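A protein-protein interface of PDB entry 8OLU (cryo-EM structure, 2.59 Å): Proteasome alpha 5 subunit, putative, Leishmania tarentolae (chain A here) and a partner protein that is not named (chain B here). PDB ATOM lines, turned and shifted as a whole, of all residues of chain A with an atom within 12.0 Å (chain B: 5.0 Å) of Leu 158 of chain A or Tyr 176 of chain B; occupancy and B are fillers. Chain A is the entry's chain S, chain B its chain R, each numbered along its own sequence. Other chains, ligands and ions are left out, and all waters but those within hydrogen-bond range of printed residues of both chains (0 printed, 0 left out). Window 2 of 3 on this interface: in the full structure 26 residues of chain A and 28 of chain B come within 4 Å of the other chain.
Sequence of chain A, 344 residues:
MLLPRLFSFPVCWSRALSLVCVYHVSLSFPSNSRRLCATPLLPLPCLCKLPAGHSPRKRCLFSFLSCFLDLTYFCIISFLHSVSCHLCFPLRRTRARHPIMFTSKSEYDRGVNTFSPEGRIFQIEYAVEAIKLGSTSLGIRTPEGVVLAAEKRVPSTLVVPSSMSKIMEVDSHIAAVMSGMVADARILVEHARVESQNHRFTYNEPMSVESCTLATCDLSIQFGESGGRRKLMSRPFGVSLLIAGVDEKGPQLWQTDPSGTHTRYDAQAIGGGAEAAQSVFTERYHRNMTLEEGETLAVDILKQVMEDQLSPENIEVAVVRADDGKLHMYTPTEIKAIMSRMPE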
ATOM      1  N   LYS A 152     -16.915  -3.159  -5.533  1.00  0.00           N
ATOM      2  CA  LYS A 152     -16.958  -2.247  -4.395  1.00  0.00           C
ATOM      3  C   LYS A 152     -16.261  -2.826  -3.154  1.00  0.00           C
ATOM      4  O   LYS A 152     -15.632  -2.079  -2.422  1.00  0.00           O
ATOM      5  CB  LYS A 152     -18.385  -1.887  -3.991  1.00  0.00           C
ATOM      6  CG  LYS A 152     -19.102  -0.894  -4.896  1.00  0.00           C
ATOM      7  CD  LYS A 152     -20.133  -0.078  -4.135  1.00  0.00           C
ATOM      8  CE  LYS A 152     -21.060   0.763  -4.990  1.00  0.00           C
ATOM      9  NZ  LYS A 152     -20.395   2.029  -5.390  1.00  0.00           N
ATOM     10  N   ARG A 153     -16.383  -4.138  -2.906  1.00  0.00           N
ATOM     11  CA  ARG A 153     -15.818  -4.798  -1.730  1.00  0.00           C
ATOM     12  C   ARG A 153     -16.147  -4.052  -0.443  1.00  0.00           C
ATOM     13  O   ARG A 153     -15.241  -3.645   0.271  1.00  0.00           O
ATOM     14  CB  ARG A 153     -14.294  -4.937  -1.833  1.00  0.00           C
ATOM     15  CG  ARG A 153     -13.675  -5.917  -0.841  1.00  0.00           C
ATOM     16  CD  ARG A 153     -12.171  -6.091  -1.003  1.00  0.00           C
ATOM     17  NE  ARG A 153     -11.802  -7.035  -2.058  1.00  0.00           N
ATOM     18  CZ  ARG A 153     -10.548  -7.296  -2.436  1.00  0.00           C
ATOM     19  NH1 ARG A 153     -10.302  -8.198  -3.380  1.00  0.00           N
ATOM     20  NH2 ARG A 153      -9.542  -6.637  -1.877  1.00  0.00           N
ATOM     21  N   VAL A 154     -17.439  -3.933  -0.113  1.00  0.00           N
ATOM     22  CA  VAL A 154     -17.836  -3.259   1.114  1.00  0.00           C
ATOM     23  C   VAL A 154     -17.574  -4.179   2.309  1.00  0.00           C
ATOM     24  O   VAL A 154     -17.711  -5.403   2.201  1.00  0.00           O
ATOM     25  CB  VAL A 154     -19.303  -2.797   1.076  1.00  0.00           C
ATOM     26  CG1 VAL A 154     -19.581  -1.899  -0.116  1.00  0.00           C
ATOM     27  CG2 VAL A 154     -20.285  -3.957   1.105  1.00  0.00           C
ATOM     28  N   PRO A 155     -17.200  -3.610   3.485  1.00  0.00           N
ATOM     29  CA  PRO A 155     -16.967  -4.392   4.704  1.00  0.00           C
ATOM     30  C   PRO A 155     -18.211  -4.714   5.539  1.00  0.00           C
ATOM     31  O   PRO A 155     -18.121  -5.383   6.574  1.00  0.00           O
ATOM     32  CB  PRO A 155     -16.041  -3.461   5.492  1.00  0.00           C
ATOM     33  CG  PRO A 155     -16.600  -2.096   5.173  1.00  0.00           C
ATOM     34  CD  PRO A 155     -16.954  -2.175   3.699  1.00  0.00           C
ATOM     35  N   SER A 156     -19.374  -4.240   5.086  1.00  0.00           N
ATOM     36  CA  SER A 156     -20.605  -4.482   5.812  1.00  0.00           C
ATOM     37  C   SER A 156     -21.802  -4.102   4.961  1.00  0.00           C
ATOM     38  O   SER A 156     -21.735  -3.181   4.155  1.00  0.00           O
ATOM     39  CB  SER A 156     -20.616  -3.720   7.117  1.00  0.00           C
ATOM     40  OG  SER A 156     -21.942  -3.520   7.606  1.00  0.00           O
ATOM     41  N   THR A 157     -22.914  -4.782   5.222  1.00  0.00           N
ATOM     42  CA  THR A 157     -24.202  -4.401   4.673  1.00  0.00           C
ATOM     43  C   THR A 157     -24.648  -3.037   5.194  1.00  0.00           C
ATOM     44  O   THR A 157     -25.437  -2.354   4.545  1.00  0.00           O
ATOM     45  CB  THR A 157     -25.237  -5.472   5.018  1.00  0.00           C
ATOM     46  OG1 THR A 157     -25.462  -5.411   6.431  1.00  0.00           O
ATOM     47  CG2 THR A 157     -24.773  -6.845   4.572  1.00  0.00           C
ATOM     48  N   LEU A 158     -24.127  -2.630   6.354  1.00  0.00           N
ATOM     49  CA  LEU A 158     -24.484  -1.345   6.947  1.00  0.00           C
ATOM     50  C   LEU A 158     -23.832  -0.178   6.228  1.00  0.00           C
ATOM     51  O   LEU A 158     -24.132   0.959   6.538  1.00  0.00           O
ATOM     52  CB  LEU A 158     -24.030  -1.340   8.397  1.00  0.00           C
ATOM     53  CG  LEU A 158     -24.780  -2.321   9.286  1.00  0.00           C
ATOM     54  CD1 LEU A 158     -24.313  -2.201  10.722  1.00  0.00           C
ATOM     55  CD2 LEU A 158     -26.256  -2.028   9.172  1.00  0.00           C
ATOM     56  N   VAL A 159     -22.909  -0.451   5.314  1.00  0.00           N
ATOM     57  CA  VAL A 159     -22.306   0.640   4.578  1.00  0.00           C
ATOM     58  C   VAL A 159     -23.292   1.113   3.534  1.00  0.00           C
ATOM     59  O   VAL A 159     -24.026   0.301   2.948  1.00  0.00           O
ATOM     60  CB  VAL A 159     -20.984   0.270   3.891  1.00  0.00           C
ATOM     61  CG1 VAL A 159     -20.555   1.401   2.963  1.00  0.00           C
ATOM     62  CG2 VAL A 159     -19.888  -0.043   4.893  1.00  0.00           C
ATOM     63  N   VAL A 160     -23.281   2.429   3.342  1.00  0.00           N
ATOM     64  CA  VAL A 160     -24.037   3.026   2.261  1.00  0.00           C
ATOM     65  C   VAL A 160     -23.179   2.916   1.009  1.00  0.00           C
ATOM     66  O   VAL A 160     -22.091   3.492   0.943  1.00  0.00           O
ATOM     67  CB  VAL A 160     -24.391   4.479   2.574  1.00  0.00           C
ATOM     68  CG1 VAL A 160     -25.036   5.157   1.385  1.00  0.00           C
ATOM     69  CG2 VAL A 160     -25.260   4.576   3.799  1.00  0.00           C
ATOM     70  N   PRO A 161     -23.545   2.115  -0.003  1.00  0.00           N
ATOM     71  CA  PRO A 161     -22.536   1.764  -1.004  1.00  0.00           C
ATOM     72  C   PRO A 161     -22.129   2.945  -1.911  1.00  0.00           C
ATOM     73  O   PRO A 161     -20.970   3.050  -2.294  1.00  0.00           O
ATOM     74  CB  PRO A 161     -23.140   0.492  -1.631  1.00  0.00           C
ATOM     75  CG  PRO A 161     -24.290   0.095  -0.693  1.00  0.00           C
ATOM     76  CD  PRO A 161     -24.828   1.424  -0.191  1.00  0.00           C
ATOM     77  N   SER A 162     -23.001   3.930  -2.150  1.00  0.00           N
ATOM     78  CA  SER A 162     -22.582   5.093  -2.931  1.00  0.00           C
ATOM     79  C   SER A 162     -21.329   5.776  -2.359  1.00  0.00           C
ATOM     80  O   SER A 162     -20.588   6.433  -3.081  1.00  0.00           O
ATOM     81  CB  SER A 162     -23.731   6.082  -3.107  1.00  0.00           C
ATOM     82  OG  SER A 162     -24.428   6.298  -1.892  1.00  0.00           O
ATOM     83  N   SER A 163     -21.084   5.624  -1.057  1.00  0.00           N
ATOM     84  CA  SER A 163     -20.042   6.345  -0.344  1.00  0.00           C
ATOM     85  C   SER A 163     -18.663   5.733  -0.557  1.00  0.00           C
ATOM     86  O   SER A 163     -17.668   6.364  -0.221  1.00  0.00           O
ATOM     87  CB  SER A 163     -20.353   6.327   1.114  1.00  0.00           C
ATOM     88  OG  SER A 163     -20.116   5.027   1.683  1.00  0.00           O
ATOM     89  N   MET A 164     -18.623   4.486  -1.044  1.00  0.00           N
ATOM     90  CA  MET A 164     -17.396   3.743  -1.263  1.00  0.00           C
ATOM     91  C   MET A 164     -17.166   3.683  -2.762  1.00  0.00           C
ATOM     92  O   MET A 164     -17.108   2.609  -3.370  1.00  0.00           O
ATOM     93  CB  MET A 164     -17.509   2.324  -0.701  1.00  0.00           C
ATOM     94  CG  MET A 164     -16.977   2.249   0.699  1.00  0.00           C
ATOM     95  SD  MET A 164     -16.589   0.562   1.206  1.00  0.00           S
ATOM     96  CE  MET A 164     -15.931   0.884   2.849  1.00  0.00           C
ATOM     97  N   ASP A 308     -17.277 -12.106  -3.059  1.00  0.00           N
ATOM     98  CA  ASP A 308     -18.717 -12.133  -2.832  1.00  0.00           C
ATOM     99  C   ASP A 308     -19.458 -12.556  -4.106  1.00  0.00           C
ATOM    100  O   ASP A 308     -18.861 -12.692  -5.174  1.00  0.00           O
ATOM    101  CB  ASP A 308     -19.205 -10.757  -2.346  1.00  0.00           C
ATOM    102  CG  ASP A 308     -18.878 -10.413  -0.894  1.00  0.00           C
ATOM    103  OD1 ASP A 308     -19.613 -10.880   0.006  1.00  0.00           O
ATOM    104  OD2 ASP A 308     -17.890  -9.688  -0.663  1.00  0.00           O
ATOM    105  N   GLU A 313     -25.272  -3.917  -6.378  1.00  0.00           N
ATOM    106  CA  GLU A 313     -24.788  -2.906  -5.436  1.00  0.00           C
ATOM    107  C   GLU A 313     -23.313  -3.157  -5.102  1.00  0.00           C
ATOM    108  O   GLU A 313     -22.590  -2.237  -4.745  1.00  0.00           O
ATOM    109  CB  GLU A 313     -25.633  -2.895  -4.152  1.00  0.00           C
ATOM    110  CG  GLU A 313     -27.042  -2.340  -4.324  1.00  0.00           C
ATOM    111  CD  GLU A 313     -28.069  -3.243  -5.007  1.00  0.00           C
ATOM    112  OE1 GLU A 313     -29.130  -2.703  -5.425  1.00  0.00           O
ATOM    113  OE2 GLU A 313     -27.834  -4.484  -5.104  1.00  0.00           O
ATOM    114  N   ASN A 314     -22.910  -4.424  -5.210  1.00  0.00           N
ATOM    115  CA  ASN A 314     -21.553  -4.901  -5.018  1.00  0.00           C
ATOM    116  C   ASN A 314     -20.566  -4.375  -6.051  1.00  0.00           C
ATOM    117  O   ASN A 314     -19.363  -4.597  -5.891  1.00  0.00           O
ATOM    118  CB  ASN A 314     -21.468  -6.418  -5.239  1.00  0.00           C
ATOM    119  CG  ASN A 314     -21.637  -7.240  -3.982  1.00  0.00           C
ATOM    120  OD1 ASN A 314     -21.780  -6.707  -2.880  1.00  0.00           O
ATOM    121  ND2 ASN A 314     -21.596  -8.554  -4.151  1.00  0.00           N
ATOM    122  N   VAL B  35     -25.903   5.420  14.831  1.00  0.00           N
ATOM    123  CA  VAL B  35     -27.066   4.812  14.235  1.00  0.00           C
ATOM    124  C   VAL B  35     -27.842   5.882  13.526  1.00  0.00           C
ATOM    125  O   VAL B  35     -28.068   6.952  14.070  1.00  0.00           O
ATOM    126  CB  VAL B  35     -27.992   4.202  15.287  1.00  0.00           C
ATOM    127  CG1 VAL B  35     -28.964   3.290  14.590  1.00  0.00           C
ATOM    128  CG2 VAL B  35     -27.207   3.441  16.338  1.00  0.00           C
ATOM    129  N   LEU B  36     -28.303   5.514  12.355  1.00  0.00           N
ATOM    130  CA  LEU B  36     -29.032   6.430  11.524  1.00  0.00           C
ATOM    131  C   LEU B  36     -30.459   5.921  11.414  1.00  0.00           C
ATOM    132  O   LEU B  36     -30.670   4.810  10.915  1.00  0.00           O
ATOM    133  CB  LEU B  36     -28.356   6.443  10.155  1.00  0.00           C
ATOM    134  CG  LEU B  36     -29.037   7.313   9.109  1.00  0.00           C
ATOM    135  CD1 LEU B  36     -28.391   8.690   9.051  1.00  0.00           C
ATOM    136  CD2 LEU B  36     -29.030   6.630   7.751  1.00  0.00           C
ATOM    137  N   GLY B  37     -31.396   6.773  11.866  1.00  0.00           N
ATOM    138  CA  GLY B  37     -32.825   6.567  11.687  1.00  0.00           C
ATOM    139  C   GLY B  37     -33.419   7.477  10.623  1.00  0.00           C
ATOM    140  O   GLY B  37     -32.686   8.096   9.861  1.00  0.00           O
ATOM    141  N   ALA B 155     -19.905   6.147   4.347  1.00  0.00           N
ATOM    142  CA  ALA B 155     -21.133   6.491   5.025  1.00  0.00           C
ATOM    143  C   ALA B 155     -21.730   5.189   5.490  1.00  0.00           C
ATOM    144  O   ALA B 155     -21.429   4.184   4.890  1.00  0.00           O
ATOM    145  CB  ALA B 155     -22.044   7.294   4.182  1.00  0.00           C
ATOM    146  N   TRP B 156     -22.406   5.205   6.643  1.00  0.00           N
ATOM    147  CA  TRP B 156     -23.014   4.007   7.142  1.00  0.00           C
ATOM    148  C   TRP B 156     -24.402   4.309   7.628  1.00  0.00           C
ATOM    149  O   TRP B 156     -24.691   5.459   7.960  1.00  0.00           O
ATOM    150  CB  TRP B 156     -22.249   3.431   8.306  1.00  0.00           C
ATOM    151  CG  TRP B 156     -20.837   3.090   8.005  1.00  0.00           C
ATOM    152  CD1 TRP B 156     -19.848   3.923   7.597  1.00  0.00           C
ATOM    153  CD2 TRP B 156     -20.233   1.830   8.221  1.00  0.00           C
ATOM    154  NE1 TRP B 156     -18.669   3.238   7.488  1.00  0.00           N
ATOM    155  CE2 TRP B 156     -18.881   1.956   7.885  1.00  0.00           C
ATOM    156  CE3 TRP B 156     -20.715   0.612   8.643  1.00  0.00           C
ATOM    157  CZ2 TRP B 156     -18.015   0.885   7.913  1.00  0.00           C
ATOM    158  CZ3 TRP B 156     -19.863  -0.456   8.672  1.00  0.00           C
ATOM    159  CH2 TRP B 156     -18.533  -0.328   8.295  1.00  0.00           C
ATOM    160  N   ARG B 157     -25.197   3.229   7.700  1.00  0.00           N
ATOM    161  CA  ARG B 157     -26.540   3.215   8.262  1.00  0.00           C
ATOM    162  C   ARG B 157     -26.411   3.031   9.771  1.00  0.00           C
ATOM    163  O   ARG B 157     -27.185   3.581  10.552  1.00  0.00           O
ATOM    164  CB  ARG B 157     -27.393   2.120   7.613  1.00  0.00           C
ATOM    165  CG  ARG B 157     -27.808   2.463   6.185  1.00  0.00           C
ATOM    166  CD  ARG B 157     -28.533   1.360   5.382  1.00  0.00           C
ATOM    167  NE  ARG B 157     -27.916   0.026   5.347  1.00  0.00           N
ATOM    168  CZ  ARG B 157     -28.520  -1.097   5.750  1.00  0.00           C
ATOM    169  NH1 ARG B 157     -27.854  -2.239   5.885  1.00  0.00           N
ATOM    170  NH2 ARG B 157     -29.814  -1.064   6.007  1.00  0.00           N
ATOM    171  N   ALA B 158     -25.405   2.267  10.170  1.00  0.00           N
ATOM    172  CA  ALA B 158     -24.967   2.289  11.548  1.00  0.00           C
ATOM    173  C   ALA B 158     -23.525   1.848  11.600  1.00  0.00           C
ATOM    174  O   ALA B 158     -23.075   1.124  10.719  1.00  0.00           O
ATOM    175  CB  ALA B 158     -25.772   1.351  12.370  1.00  0.00           C
ATOM    176  N   ILE B 169     -20.359  -4.449  14.944  1.00  0.00           N
ATOM    177  CA  ILE B 169     -20.862  -4.233  13.595  1.00  0.00           C
ATOM    178  C   ILE B 169     -21.556  -5.498  13.097  1.00  0.00           C
ATOM    179  O   ILE B 169     -22.586  -5.386  12.458  1.00  0.00           O
ATOM    180  CB  ILE B 169     -19.726  -3.761  12.664  1.00  0.00           C
ATOM    181  CG1 ILE B 169     -19.437  -2.264  12.851  1.00  0.00           C
ATOM    182  CG2 ILE B 169     -19.999  -4.087  11.203  1.00  0.00           C
ATOM    183  CD1 ILE B 169     -18.256  -1.734  12.026  1.00  0.00           C
ATOM    184  N   MET B 172     -24.947  -5.463  14.633  1.00  0.00           N
ATOM    185  CA  MET B 172     -25.827  -4.467  14.073  1.00  0.00           C
ATOM    186  C   MET B 172     -26.265  -4.902  12.679  1.00  0.00           C
ATOM    187  O   MET B 172     -27.345  -4.520  12.243  1.00  0.00           O
ATOM    188  CB  MET B 172     -25.126  -3.106  14.029  1.00  0.00           C
ATOM    189  CG  MET B 172     -24.818  -2.552  15.422  1.00  0.00           C
ATOM    190  SD  MET B 172     -24.296  -0.800  15.545  1.00  0.00           S
ATOM    191  CE  MET B 172     -23.100  -0.603  14.231  1.00  0.00           C
ATOM    192  N   GLU B 173     -25.458  -5.693  11.960  1.00  0.00           N
ATOM    193  CA  GLU B 173     -25.848  -6.083  10.612  1.00  0.00           C
ATOM    194  C   GLU B 173     -27.132  -6.898  10.723  1.00  0.00           C
ATOM    195  O   GLU B 173     -28.116  -6.623  10.040  1.00  0.00           O
ATOM    196  CB  GLU B 173     -24.745  -6.880   9.905  1.00  0.00           C
ATOM    197  CG  GLU B 173     -23.620  -6.034   9.303  1.00  0.00           C
ATOM    198  CD  GLU B 173     -22.304  -6.751   8.998  1.00  0.00           C
ATOM    199  OE1 GLU B 173     -22.209  -7.981   9.251  1.00  0.00           O
ATOM    200  OE2 GLU B 173     -21.358  -6.080   8.518  1.00  0.00           O
ATOM    201  N   LYS B 174     -27.112  -7.849  11.665  1.00  0.00           N
ATOM    202  CA  LYS B 174     -28.233  -8.738  11.913  1.00  0.00           C
ATOM    203  C   LYS B 174     -29.517  -7.949  12.192  1.00  0.00           C
ATOM    204  O   LYS B 174     -30.430  -7.990  11.376  1.00  0.00           O
ATOM    205  CB  LYS B 174     -27.823  -9.744  12.989  1.00  0.00           C
ATOM    206  CG  LYS B 174     -26.830 -10.778  12.462  1.00  0.00           C
ATOM    207  CD  LYS B 174     -26.846 -12.105  13.207  1.00  0.00           C
ATOM    208  CE  LYS B 174     -26.212 -12.025  14.583  1.00  0.00           C
ATOM    209  NZ  LYS B 174     -24.751 -11.769  14.501  1.00  0.00           N
ATOM    210  N   SER B 175     -29.563  -7.203  13.297  1.00  0.00           N
ATOM    211  CA  SER B 175     -30.770  -6.504  13.727  1.00  0.00           C
ATOM    212  C   SER B 175     -31.212  -5.401  12.752  1.00  0.00           C
ATOM    213  O   SER B 175     -32.317  -5.457  12.220  1.00  0.00           O
ATOM    214  CB  SER B 175     -30.574  -5.926  15.107  1.00  0.00           C
ATOM    215  OG  SER B 175     -29.606  -6.674  15.849  1.00  0.00           O
ATOM    216  N   TYR B 176     -30.332  -4.423  12.502  1.00  0.00           N
ATOM    217  CA  TYR B 176     -30.668  -3.058  12.109  1.00  0.00           C
ATOM    218  C   TYR B 176     -31.686  -3.000  10.973  1.00  0.00           C
ATOM    219  O   TYR B 176     -31.453  -3.595   9.924  1.00  0.00           O
ATOM    220  CB  TYR B 176     -29.399  -2.330  11.636  1.00  0.00           C
ATOM    221  CG  TYR B 176     -29.630  -0.974  11.008  1.00  0.00           C
ATOM    222  CD1 TYR B 176     -29.546   0.184  11.752  1.00  0.00           C
ATOM    223  CD2 TYR B 176     -29.943  -0.841   9.677  1.00  0.00           C
ATOM    224  CE1 TYR B 176     -29.794   1.424  11.201  1.00  0.00           C
ATOM    225  CE2 TYR B 176     -30.212   0.395   9.109  1.00  0.00           C
ATOM    226  CZ  TYR B 176     -30.145   1.536   9.872  1.00  0.00           C
ATOM    227  OH  TYR B 176     -30.382   2.768   9.294  1.00  0.00           O
ATOM    228  N   LYS B 177     -32.764  -2.207  11.158  1.00  0.00           N
ATOM    229  CA  LYS B 177     -33.721  -1.956  10.083  1.00  0.00           C
ATOM    230  C   LYS B 177     -33.655  -0.489   9.709  1.00  0.00           C
ATOM    231  O   LYS B 177     -33.355   0.348  10.560  1.00  0.00           O
ATOM    232  CB  LYS B 177     -35.188  -2.224  10.455  1.00  0.00           C
ATOM    233  CG  LYS B 177     -35.629  -3.683  10.563  1.00  0.00           C
ATOM    234  CD  LYS B 177     -35.210  -4.352  11.879  1.00  0.00           C
ATOM    235  CE  LYS B 177     -35.837  -3.774  13.137  1.00  0.00           C
ATOM    236  NZ  LYS B 177     -36.976  -4.596  13.609  1.00  0.00           N
ATOM    237  N   ASP B 178     -34.008  -0.195   8.453  1.00  0.00           N
ATOM    238  CA  ASP B 178     -34.169   1.179   8.002  1.00  0.00           C
ATOM    239  C   ASP B 178     -35.356   1.815   8.730  1.00  0.00           C
ATOM    240  O   ASP B 178     -36.120   1.135   9.422  1.00  0.00           O
ATOM    241  CB  ASP B 178     -34.307   1.287   6.472  1.00  0.00           C
ATOM    242  CG  ASP B 178     -33.104   0.812   5.654  1.00  0.00           C
ATOM    243  OD1 ASP B 178     -32.028   1.460   5.718  1.00  0.00           O
ATOM    244  OD2 ASP B 178     -33.251  -0.210   4.947  1.00  0.00           O
ATOM    245  N   MET B 180     -35.991   3.656  11.416  1.00  0.00           N
ATOM    246  CA  MET B 180     -36.289   3.565  12.829  1.00  0.00           C
ATOM    247  C   MET B 180     -36.790   4.927  13.279  1.00  0.00           C
ATOM    248  O   MET B 180     -36.643   5.895  12.543  1.00  0.00           O
ATOM    249  CB  MET B 180     -35.073   3.135  13.656  1.00  0.00           C
ATOM    250  CG  MET B 180     -34.949   1.604  13.742  1.00  0.00           C
ATOM    251  SD  MET B 180     -33.497   0.888  14.615  1.00  0.00           S
ATOM    252  CE  MET B 180     -32.183   1.946  14.003  1.00  0.00           C
ATOM    253  N   PHE B 188     -31.577   1.035  19.858  1.00  0.00           N
ATOM    254  CA  PHE B 188     -30.759   0.147  19.056  1.00  0.00           C
ATOM    255  C   PHE B 188     -29.282   0.376  19.337  1.00  0.00           C
ATOM    256  O   PHE B 188     -28.496  -0.568  19.330  1.00  0.00           O
ATOM    257  CB  PHE B 188     -30.962   0.447  17.585  1.00  0.00           C
ATOM    258  CG  PHE B 188     -30.122  -0.436  16.723  1.00  0.00           C
ATOM    259  CD1 PHE B 188     -28.975   0.046  16.116  1.00  0.00           C
ATOM    260  CD2 PHE B 188     -30.484  -1.753  16.528  1.00  0.00           C
ATOM    261  CE1 PHE B 188     -28.204  -0.776  15.312  1.00  0.00           C
ATOM    262  CE2 PHE B 188     -29.731  -2.561  15.703  1.00  0.00           C
ATOM    263  CZ  PHE B 188     -28.590  -2.078  15.105  1.00  0.00           C
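The backbone carbonyl oxygen (O) of Leu 36 of chain B sits at hydrogen-bond distance from the side-chain hydroxyl (OH) of Tyr 176 of chain B (2.6 Å). The side-chain carboxylate of Asp 178 of chain B is in salt-bridge range of the guanidinium group of Arg 157 of chain B. The backbone carbonyl oxygen of Arg 157 of chain B is in hydrogen-bond range of the backbone NH of Leu 36 of chain B. OG of Ser 156 of chain A sits at hydrogen-bond distance from N of Leu 158 of chain A (2.7 Å). OG of Ser 163 of chain A lies within hydrogen-bond range of O of Val 160 of chain A (2.6 Å).
O of Leu 158 of chain A is in hydrogen-bond range of N of Arg 157 of chain B, at 2.8 Å. OE2 of Glu 173 of chain B lies within hydrogen-bond range of OG of Ser 156 of chain A (2.8 Å). The guanidinium group of Arg 157 of chain B is in hydrogen-bond range of the backbone carbonyl oxygen of Thr 157 of chain A. The backbone NH of Val 160 of chain A lies within hydrogen-bond range of the backbone carbonyl oxygen of Ala 155 of chain B (3.0 Å). The side-chain hydroxyl (OG) of Ser 163 of chain A sits at hydrogen-bond distance from the backbone NH (N) of Ala 155 of chain B.
Of the printed residues of chain B, Thr 157 of chain A touches Arg 157 (2.8 Å) and Glu 173 (3.5 Å). Of the printed residues of chain B, Leu 158 of chain A touches Trp 156 (3.3 Å), Arg 157 (2.8 Å), Ala 158 (3.5 Å), Met 172 (3.5 Å), Glu 173 (3.9 Å) and Tyr 176 (3.9 Å). Of the printed residues of chain B, Val 159 of chain A touches Ala 155 (3.5 Å) and Trp 156 (3.7 Å). Of the printed residues of chain B, Val 160 of chain A touches Ala 155 and Trp 156. Printed residues of chain B within 4 Å of Ser 163 of chain A: Ala 155 (2.9 Å). No residue of chain A comes within 4 Å of Val 35 of chain B. No residue of chain A comes within 4 Å of Leu 36 of chain B. Trp 156 of chain B touches just these residues of chain A: Ser 156 (3.7 Å), Leu 158 (3.3 Å), Val 159 (3.7 Å) and Val 160 (3.9 Å). Of the printed residues of chain A, Ala 158 of chain B touches Leu 158 (3.5 Å). Of chain A, only Leu 158 (3.5 Å) comes within 4 Å of Met 172 of chain B. Glu 173 of chain B touches just these residues of chain A: Pro 155 (3.8 Å), Ser 156 (2.8 Å), Thr 157 (3.5 Å) and Leu 158 (3.9 Å). No residue of chain A comes within 4 Å of Ser 175 of chain B. Of chain A, only Leu 158 (3.9 Å) comes within 4 Å of Tyr 176 of chain B. Lys 177 of chain B touches none of the printed residues of chain A. No residue of chain A comes within 4 Å of Asp 178 of chain B.
Among the printed residues, merely in contact across the chains: Leu 158 of chain A with Trp 156 of chain B (3.3 Å), Thr 157 of chain A with Glu 173 of chain B (3.5 Å), Val 159 of chain A with Ala 155 of chain B (3.5 Å), Leu 158 of chain A with Ala 158 of chain B (3.5 Å), Leu 158 of chain A with Met 172 of chain B (3.5 Å), Val 159 of chain A with Trp 156 of chain B (3.7 Å), Ser 156 of chain A with Trp 156 of chain B (3.7 Å), Pro 155 of chain A with Glu 173 of chain B (3.8 Å), Leu 158 of chain A with Glu 173 of chain B (3.9 Å), Leu 158 of chain A with Tyr 176 of chain B (3.9 Å) and Val 160 of chain A with Trp 156 of chain B (3.9 Å).
Printed residues of chain B that touch a printed residue of chain A: Ala 155, Trp 156, Arg 157, Ala 158, Met 172, Glu 173 and Tyr 176. Hydrophobic or aromatic side chains of chain A within 4 Å of the printed part of chain B: Leu 158, Val 159 and Val 160. Among the printed residues, no Asp or Glu carboxylate lies within 4 Å of a Lys or Arg side-chain nitrogen of the other chain.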
